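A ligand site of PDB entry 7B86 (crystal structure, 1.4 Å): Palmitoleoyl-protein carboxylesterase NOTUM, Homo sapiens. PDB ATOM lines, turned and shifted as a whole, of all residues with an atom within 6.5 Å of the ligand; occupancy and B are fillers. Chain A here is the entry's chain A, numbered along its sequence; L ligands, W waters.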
ATOM      1  N   GLY A  49      13.773   4.861  -5.896  1.00  0.00           N
ATOM      2  CA  GLY A  49      13.523   3.435  -5.884  1.00  0.00           C
ATOM      3  C   GLY A  49      12.404   3.021  -4.922  1.00  0.00           C
ATOM      4  O   GLY A  49      11.600   3.839  -4.462  1.00  0.00           O
ATOM      5  N   GLY A  50      12.318   1.695  -4.698  1.00  0.00           N
ATOM      6  CA  GLY A  50      11.313   1.134  -3.808  1.00  0.00           C
ATOM      7  C   GLY A  50      10.594  -0.111  -4.336  1.00  0.00           C
ATOM      8  O   GLY A  50       9.374  -0.097  -4.462  1.00  0.00           O
ATOM      9  N   TRP A  51      11.345  -1.169  -4.635  1.00  0.00           N
ATOM     10  CA  TRP A  51      10.796  -2.477  -5.068  1.00  0.00           C
ATOM     11  C   TRP A  51       9.946  -2.307  -6.343  1.00  0.00           C
ATOM     12  O   TRP A  51      10.315  -1.505  -7.214  1.00  0.00           O
ATOM     13  CB  TRP A  51      10.161  -3.224  -3.893  1.00  0.00           C
ATOM     14  CG  TRP A  51      11.182  -3.597  -2.856  1.00  0.00           C
ATOM     15  CD1 TRP A  51      11.497  -2.904  -1.721  1.00  0.00           C
ATOM     16  CD2 TRP A  51      12.080  -4.722  -2.894  1.00  0.00           C
ATOM     17  NE1 TRP A  51      12.515  -3.543  -1.039  1.00  0.00           N
ATOM     18  CE2 TRP A  51      12.892  -4.657  -1.749  1.00  0.00           C
ATOM     19  CE3 TRP A  51      12.270  -5.775  -3.790  1.00  0.00           C
ATOM     20  CZ2 TRP A  51      13.867  -5.608  -1.464  1.00  0.00           C
ATOM     21  CZ3 TRP A  51      13.245  -6.719  -3.520  1.00  0.00           C
ATOM     22  CH2 TRP A  51      14.030  -6.631  -2.364  1.00  0.00           C
ATOM     23  N   TYR A  52       8.843  -3.052  -6.459  1.00  0.00           N
ATOM     24  CA  TYR A  52       8.001  -3.146  -7.655  1.00  0.00           C
ATOM     25  C   TYR A  52       6.841  -4.069  -7.323  1.00  0.00           C
ATOM     26  O   TYR A  52       6.815  -4.698  -6.266  1.00  0.00           O
ATOM     27  CB  TYR A  52       8.793  -3.665  -8.880  1.00  0.00           C
ATOM     28  CG  TYR A  52       9.425  -5.048  -8.737  1.00  0.00           C
ATOM     29  CD1 TYR A  52       8.721  -6.214  -9.082  1.00  0.00           C
ATOM     30  CD2 TYR A  52      10.742  -5.194  -8.312  1.00  0.00           C
ATOM     31  CE1 TYR A  52       9.307  -7.464  -8.977  1.00  0.00           C
ATOM     32  CE2 TYR A  52      11.321  -6.458  -8.188  1.00  0.00           C
ATOM     33  CZ  TYR A  52      10.603  -7.577  -8.536  1.00  0.00           C
ATOM     34  OH  TYR A  52      11.183  -8.828  -8.419  1.00  0.00           O
ATOM     35  N   TYR A 105       9.157   7.781  -8.035  1.00  0.00           N
ATOM     36  CA  TYR A 105       8.888   6.452  -8.583  1.00  0.00           C
ATOM     37  C   TYR A 105       7.435   6.122  -8.274  1.00  0.00           C
ATOM     38  O   TYR A 105       7.088   5.798  -7.133  1.00  0.00           O
ATOM     39  CB  TYR A 105       9.830   5.453  -7.924  1.00  0.00           C
ATOM     40  CG  TYR A 105       9.758   3.987  -8.335  1.00  0.00           C
ATOM     41  CD1 TYR A 105       9.604   3.609  -9.654  1.00  0.00           C
ATOM     42  CD2 TYR A 105       9.930   2.982  -7.362  1.00  0.00           C
ATOM     43  CE1 TYR A 105       9.607   2.247 -10.024  1.00  0.00           C
ATOM     44  CE2 TYR A 105       9.920   1.636  -7.705  1.00  0.00           C
ATOM     45  CZ  TYR A 105       9.752   1.271  -9.031  1.00  0.00           C
ATOM     46  OH  TYR A 105       9.750  -0.065  -9.369  1.00  0.00           O
ATOM     47  N   VAL A 110      10.299  -0.949 -12.067  1.00  0.00           N
ATOM     48  CA  VAL A 110      11.745  -0.758 -12.205  1.00  0.00           C
ATOM     49  C   VAL A 110      12.084   0.200 -13.347  1.00  0.00           C
ATOM     50  O   VAL A 110      13.138   0.078 -13.992  1.00  0.00           O
ATOM     51  CB  VAL A 110      12.492  -2.114 -12.313  1.00  0.00           C
ATOM     52  CG1 VAL A 110      13.968  -1.937 -11.870  1.00  0.00           C
ATOM     53  CG2 VAL A 110      11.808  -3.197 -11.475  1.00  0.00           C
ATOM     54  N   SER A 154      18.754   5.242  -7.163  1.00  0.00           N
ATOM     55  CA  SER A 154      19.065   4.291  -6.078  1.00  0.00           C
ATOM     56  C   SER A 154      18.080   3.128  -6.066  1.00  0.00           C
ATOM     57  O   SER A 154      16.871   3.315  -6.243  1.00  0.00           O
ATOM     58  CB  SER A 154      19.082   4.975  -4.694  1.00  0.00           C
ATOM     59  OG  SER A 154      20.121   5.957  -4.594  1.00  0.00           O
ATOM     60  N   SER A 155      18.621   1.902  -5.847  1.00  0.00           N
ATOM     61  CA  SER A 155      17.862   0.641  -5.744  1.00  0.00           C
ATOM     62  C   SER A 155      17.097   0.385  -7.025  1.00  0.00           C
ATOM     63  O   SER A 155      17.756   0.214  -8.084  1.00  0.00           O
ATOM     64  CB  SER A 155      17.088   0.544  -4.414  1.00  0.00           C
ATOM     65  OG  SER A 155      15.825   1.164  -4.488  1.00  0.00           O
ATOM     66  N   ALA A 156      15.756   0.305  -7.046  1.00  0.00           N
ATOM     67  CA  ALA A 156      15.044   0.162  -8.311  1.00  0.00           C
ATOM     68  C   ALA A 156      15.379   1.299  -9.279  1.00  0.00           C
ATOM     69  O   ALA A 156      15.361   1.105 -10.501  1.00  0.00           O
ATOM     70  CB  ALA A 156      13.526   0.063  -8.084  1.00  0.00           C
ATOM     71  N   GLY A 157      15.701   2.489  -8.746  1.00  0.00           N
ATOM     72  CA  GLY A 157      16.136   3.576  -9.598  1.00  0.00           C
ATOM     73  C   GLY A 157      17.545   3.379 -10.136  1.00  0.00           C
ATOM     74  O   GLY A 157      17.871   3.879 -11.226  1.00  0.00           O
ATOM     75  N   THR A 159      18.819   0.313 -10.969  1.00  0.00           N
ATOM     76  CA  THR A 159      18.569  -0.542 -12.130  1.00  0.00           C
ATOM     77  C   THR A 159      17.934   0.268 -13.259  1.00  0.00           C
ATOM     78  O   THR A 159      18.264   0.081 -14.444  1.00  0.00           O
ATOM     79  CB  THR A 159      17.693  -1.748 -11.732  1.00  0.00           C
ATOM     80  OG1 THR A 159      18.229  -2.369 -10.544  1.00  0.00           O
ATOM     81  CG2 THR A 159      17.622  -2.789 -12.842  1.00  0.00           C
ATOM     82  N   SER A 188      23.203   0.925  -5.894  1.00  0.00           N
ATOM     83  CA  SER A 188      22.474  -0.137  -5.192  1.00  0.00           C
ATOM     84  C   SER A 188      21.470  -0.865  -6.092  1.00  0.00           C
ATOM     85  O   SER A 188      20.434  -1.372  -5.610  1.00  0.00           O
ATOM     86  CB  SER A 188      21.839   0.398  -3.903  1.00  0.00           C
ATOM     87  OG  SER A 188      22.842   0.893  -2.998  1.00  0.00           O
ATOM     88  N   GLY A 189      21.779  -0.942  -7.384  1.00  0.00           N
ATOM     89  CA  GLY A 189      20.925  -1.604  -8.351  1.00  0.00           C
ATOM     90  C   GLY A 189      21.605  -2.702  -9.153  1.00  0.00           C
ATOM     91  O   GLY A 189      21.068  -3.106 -10.199  1.00  0.00           O
ATOM     92  N   PHE A 191      22.557  -6.428  -9.093  1.00  0.00           N
ATOM     93  CA  PHE A 191      22.204  -7.660  -8.393  1.00  0.00           C
ATOM     94  C   PHE A 191      22.740  -8.893  -9.123  1.00  0.00           C
ATOM     95  O   PHE A 191      23.105  -8.850 -10.302  1.00  0.00           O
ATOM     96  CB  PHE A 191      20.671  -7.760  -8.198  1.00  0.00           C
ATOM     97  CG  PHE A 191      20.114  -6.636  -7.360  1.00  0.00           C
ATOM     98  CD1 PHE A 191      19.315  -5.651  -7.925  1.00  0.00           C
ATOM     99  CD2 PHE A 191      20.472  -6.528  -6.023  1.00  0.00           C
ATOM    100  CE1 PHE A 191      18.832  -4.604  -7.150  1.00  0.00           C
ATOM    101  CE2 PHE A 191      19.996  -5.475  -5.251  1.00  0.00           C
ATOM    102  CZ  PHE A 191      19.168  -4.512  -5.827  1.00  0.00           C
ATOM    103  N   PRO A 210      13.367 -16.419  -7.762  1.00  0.00           N
ATOM    104  CA  PRO A 210      12.911 -15.027  -7.654  1.00  0.00           C
ATOM    105  C   PRO A 210      13.142 -14.231  -8.941  1.00  0.00           C
ATOM    106  O   PRO A 210      12.535 -13.162  -9.080  1.00  0.00           O
ATOM    107  CB  PRO A 210      13.739 -14.470  -6.500  1.00  0.00           C
ATOM    108  CG  PRO A 210      14.959 -15.324  -6.453  1.00  0.00           C
ATOM    109  CD  PRO A 210      14.508 -16.701  -6.862  1.00  0.00           C
ATOM    110  N   THR A 211      13.993 -14.713  -9.856  1.00  0.00           N
ATOM    111  CA  THR A 211      14.024 -14.148 -11.199  1.00  0.00           C
ATOM    112  C   THR A 211      12.682 -14.344 -11.901  1.00  0.00           C
ATOM    113  O   THR A 211      12.394 -13.643 -12.881  1.00  0.00           O
ATOM    114  CB  THR A 211      15.112 -14.801 -12.064  1.00  0.00           C
ATOM    115  OG1 THR A 211      14.932 -16.227 -12.078  1.00  0.00           O
ATOM    116  CG2 THR A 211      16.488 -14.452 -11.565  1.00  0.00           C
ATOM    117  N   ILE A 214      10.614 -11.046 -11.887  1.00  0.00           N
ATOM    118  CA  ILE A 214      10.969 -10.096 -12.956  1.00  0.00           C
ATOM    119  C   ILE A 214      10.401 -10.557 -14.291  1.00  0.00           C
ATOM    120  O   ILE A 214       9.860  -9.758 -15.062  1.00  0.00           O
ATOM    121  CB  ILE A 214      12.496  -9.882 -13.008  1.00  0.00           C
ATOM    122  CG1 ILE A 214      12.992  -9.162 -11.748  1.00  0.00           C
ATOM    123  CG2 ILE A 214      12.882  -9.099 -14.284  1.00  0.00           C
ATOM    124  CD1 ILE A 214      12.440  -7.749 -11.578  1.00  0.00           C
ATOM    125  N   TRP A 239      14.473 -10.663 -19.265  1.00  0.00           N
ATOM    126  CA  TRP A 239      14.777 -10.551 -17.836  1.00  0.00           C
ATOM    127  C   TRP A 239      16.280 -10.467 -17.572  1.00  0.00           C
ATOM    128  O   TRP A 239      16.688  -9.844 -16.587  1.00  0.00           O
ATOM    129  CB  TRP A 239      14.166 -11.742 -17.056  1.00  0.00           C
ATOM    130  CG  TRP A 239      14.801 -13.091 -17.370  1.00  0.00           C
ATOM    131  CD1 TRP A 239      14.380 -13.986 -18.305  1.00  0.00           C
ATOM    132  CD2 TRP A 239      15.982 -13.657 -16.771  1.00  0.00           C
ATOM    133  NE1 TRP A 239      15.229 -15.088 -18.319  1.00  0.00           N
ATOM    134  CE2 TRP A 239      16.209 -14.902 -17.388  1.00  0.00           C
ATOM    135  CE3 TRP A 239      16.865 -13.218 -15.782  1.00  0.00           C
ATOM    136  CZ2 TRP A 239      17.296 -15.730 -17.039  1.00  0.00           C
ATOM    137  CZ3 TRP A 239      17.946 -14.035 -15.428  1.00  0.00           C
ATOM    138  CH2 TRP A 239      18.144 -15.272 -16.060  1.00  0.00           C
ATOM    139  N   PHE A 242      17.891  -7.005 -16.761  1.00  0.00           N
ATOM    140  CA  PHE A 242      17.714  -6.354 -15.454  1.00  0.00           C
ATOM    141  C   PHE A 242      18.892  -6.623 -14.517  1.00  0.00           C
ATOM    142  O   PHE A 242      18.933  -6.052 -13.404  1.00  0.00           O
ATOM    143  CB  PHE A 242      16.401  -6.817 -14.788  1.00  0.00           C
ATOM    144  CG  PHE A 242      15.147  -6.166 -15.340  1.00  0.00           C
ATOM    145  CD1 PHE A 242      14.780  -6.314 -16.676  1.00  0.00           C
ATOM    146  CD2 PHE A 242      14.301  -5.438 -14.506  1.00  0.00           C
ATOM    147  CE1 PHE A 242      13.611  -5.713 -17.170  1.00  0.00           C
ATOM    148  CE2 PHE A 242      13.139  -4.843 -14.996  1.00  0.00           C
ATOM    149  CZ  PHE A 242      12.801  -4.982 -16.316  1.00  0.00           C
ATOM    150  N   PHE A 243      19.853  -7.445 -14.923  1.00  0.00           N
ATOM    151  CA  PHE A 243      21.004  -7.771 -14.102  1.00  0.00           C
ATOM    152  C   PHE A 243      22.218  -6.989 -14.610  1.00  0.00           C
ATOM    153  O   PHE A 243      22.634  -7.159 -15.762  1.00  0.00           O
ATOM    154  CB  PHE A 243      21.226  -9.290 -14.082  1.00  0.00           C
ATOM    155  CG  PHE A 243      20.178 -10.006 -13.252  1.00  0.00           C
ATOM    156  CD1 PHE A 243      18.963 -10.367 -13.809  1.00  0.00           C
ATOM    157  CD2 PHE A 243      20.386 -10.214 -11.903  1.00  0.00           C
ATOM    158  CE1 PHE A 243      17.981 -10.963 -13.038  1.00  0.00           C
ATOM    159  CE2 PHE A 243      19.411 -10.829 -11.121  1.00  0.00           C
ATOM    160  CZ  PHE A 243      18.216 -11.189 -11.691  1.00  0.00           C
ATOM    161  N   GLY A 244      22.744  -6.113 -13.749  1.00  0.00           N
ATOM    162  CA  GLY A 244      23.782  -5.168 -14.145  1.00  0.00           C
ATOM    163  C   GLY A 244      24.944  -5.798 -14.911  1.00  0.00           C
ATOM    164  O   GLY A 244      25.379  -5.269 -15.930  1.00  0.00           O
ATOM    165  N   ASP A 263      25.080  -6.301  -0.040  1.00  0.00           N
ATOM    166  CA  ASP A 263      23.882  -5.476  -0.037  1.00  0.00           C
ATOM    167  C   ASP A 263      22.725  -6.199   0.676  1.00  0.00           C
ATOM    168  O   ASP A 263      22.483  -7.379   0.422  1.00  0.00           O
ATOM    169  CB  ASP A 263      23.521  -5.142  -1.485  1.00  0.00           C
ATOM    170  CG  ASP A 263      22.284  -4.303  -1.615  1.00  0.00           C
ATOM    171  OD1 ASP A 263      22.399  -3.061  -1.701  1.00  0.00           O
ATOM    172  OD2 ASP A 263      21.188  -4.894  -1.658  1.00  0.00           O
ATOM    173  N   ALA A 265      19.491  -5.987   0.427  1.00  0.00           N
ATOM    174  CA  ALA A 265      18.405  -6.492  -0.411  1.00  0.00           C
ATOM    175  C   ALA A 265      18.804  -7.762  -1.138  1.00  0.00           C
ATOM    176  O   ALA A 265      17.993  -8.677  -1.286  1.00  0.00           O
ATOM    177  CB  ALA A 265      17.944  -5.418  -1.399  1.00  0.00           C
ATOM    178  N   GLN A 266      20.063  -7.838  -1.611  1.00  0.00           N
ATOM    179  CA  GLN A 266      20.581  -9.087  -2.182  1.00  0.00           C
ATOM    180  C   GLN A 266      20.495 -10.226  -1.168  1.00  0.00           C
ATOM    181  O   GLN A 266      20.020 -11.321  -1.494  1.00  0.00           O
ATOM    182  CB  GLN A 266      22.018  -8.867  -2.671  1.00  0.00           C
ATOM    183  CG  GLN A 266      22.714 -10.125  -3.210  1.00  0.00           C
ATOM    184  CD  GLN A 266      22.332 -10.448  -4.642  1.00  0.00           C
ATOM    185  OE1 GLN A 266      22.392  -9.583  -5.524  1.00  0.00           O
ATOM    186  NE2 GLN A 266      21.946 -11.705  -4.893  1.00  0.00           N
ATOM    187  N   VAL A 269      16.735 -11.415  -0.649  1.00  0.00           N
ATOM    188  CA  VAL A 269      16.239 -12.316  -1.681  1.00  0.00           C
ATOM    189  C   VAL A 269      16.955 -13.675  -1.636  1.00  0.00           C
ATOM    190  O   VAL A 269      16.387 -14.693  -2.047  1.00  0.00           O
ATOM    191  CB  VAL A 269      16.278 -11.659  -3.076  1.00  0.00           C
ATOM    192  CG1 VAL A 269      15.427 -10.385  -3.090  1.00  0.00           C
ATOM    193  CG2 VAL A 269      17.691 -11.361  -3.515  1.00  0.00           C
HETATM  194  N1  LIG L   1      14.146  -1.847  -3.885  1.00  0.00           N
HETATM  195  N2  LIG L   1      16.596  -8.606 -10.272  1.00  0.00           N
HETATM  196  C1  LIG L   1      16.414  -3.138  -3.317  1.00  0.00           C
HETATM  197  C2  LIG L   1      14.670  -3.695  -6.911  1.00  0.00           C
HETATM  198  C3  LIG L   1      14.302  -5.005  -6.695  1.00  0.00           C
HETATM  199  C4  LIG L   1      14.786  -6.000  -7.523  1.00  0.00           C
HETATM  200  C5  LIG L   1      15.609  -5.670  -8.597  1.00  0.00           C
HETATM  201  C6  LIG L   1      15.494  -3.360  -7.976  1.00  0.00           C
HETATM  202  C7  LIG L   1      17.212  -7.696 -11.031  1.00  0.00           C
HETATM  203  C8  LIG L   1      15.814  -2.376  -2.329  1.00  0.00           C
HETATM  204  C9  LIG L   1      14.630  -1.716  -2.648  1.00  0.00           C
HETATM  205  C10 LIG L   1      14.756  -2.594  -4.802  1.00  0.00           C
HETATM  206  N3  LIG L   1      15.876  -3.230  -4.516  1.00  0.00           N
HETATM  207  O1  LIG L   1      14.174  -2.677  -6.073  1.00  0.00           O
HETATM  208  C11 LIG L   1      15.978  -4.348  -8.820  1.00  0.00           C
HETATM  209  C12 LIG L   1      16.107  -6.661  -9.416  1.00  0.00           C
HETATM  210  C13 LIG L   1      16.926  -6.449 -10.527  1.00  0.00           C
HETATM  211  N4  LIG L   1      15.922  -7.952  -9.277  1.00  0.00           N
HETATM  212  O   HOH W   1      19.609  -2.386  -3.058  1.00  0.00           O
HETATM  213  O   HOH W   2      13.542  -9.392  -8.185  1.00  0.00           O
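A nitrogen (N1) of the ligand sits at hydrogen-bond distance from the backbone NH (N) of Trp 51 (3.0 Å).
A nitrogen (N1) of the ligand sits at hydrogen-bond distance from the side-chain hydroxyl (OG) of Ser 155, at 3.5 Å.
The backbone carbonyl oxygen of Trp 51 is in hydrogen-bond range of the side-chain hydroxyl of Tyr 105 (2.7 Å).
The backbone NH of Ala 265 lies within hydrogen-bond range of the side-chain carboxylate of Asp 263.
OG1 of Thr 159 is in hydrogen-bond range of O of Gly 189, 3.0 Å away.
Gly 50 touches the ligand.
Tyr 52 touches the ligand.
CB of Ala 156 touches O1 of the ligand, at 3.5 Å.
Thr 159 touches the ligand.
Phe 191 touches the ligand.
Ile 214 touches the ligand.
Phe 242 touches the ligand.
Phe 243 touches the ligand.
CB of Ala 265 touches C1 of the ligand, 3.3 Å away.
Hydrophobic or aromatic side chains that line the ligand: Trp 51, Tyr 52, Ala 156, Phe 191, Ile 214, Phe 242, Phe 243 and Ala 265.
Water W2 lies within hydrogen-bond range of OH of Tyr 52 (2.4 Å) and N4 of the ligand (3.0 Å).
Water W1 bridges the backbone carbonyl oxygen (O) of Ser 188 and the side-chain carboxylate (OD1) of Asp 263.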
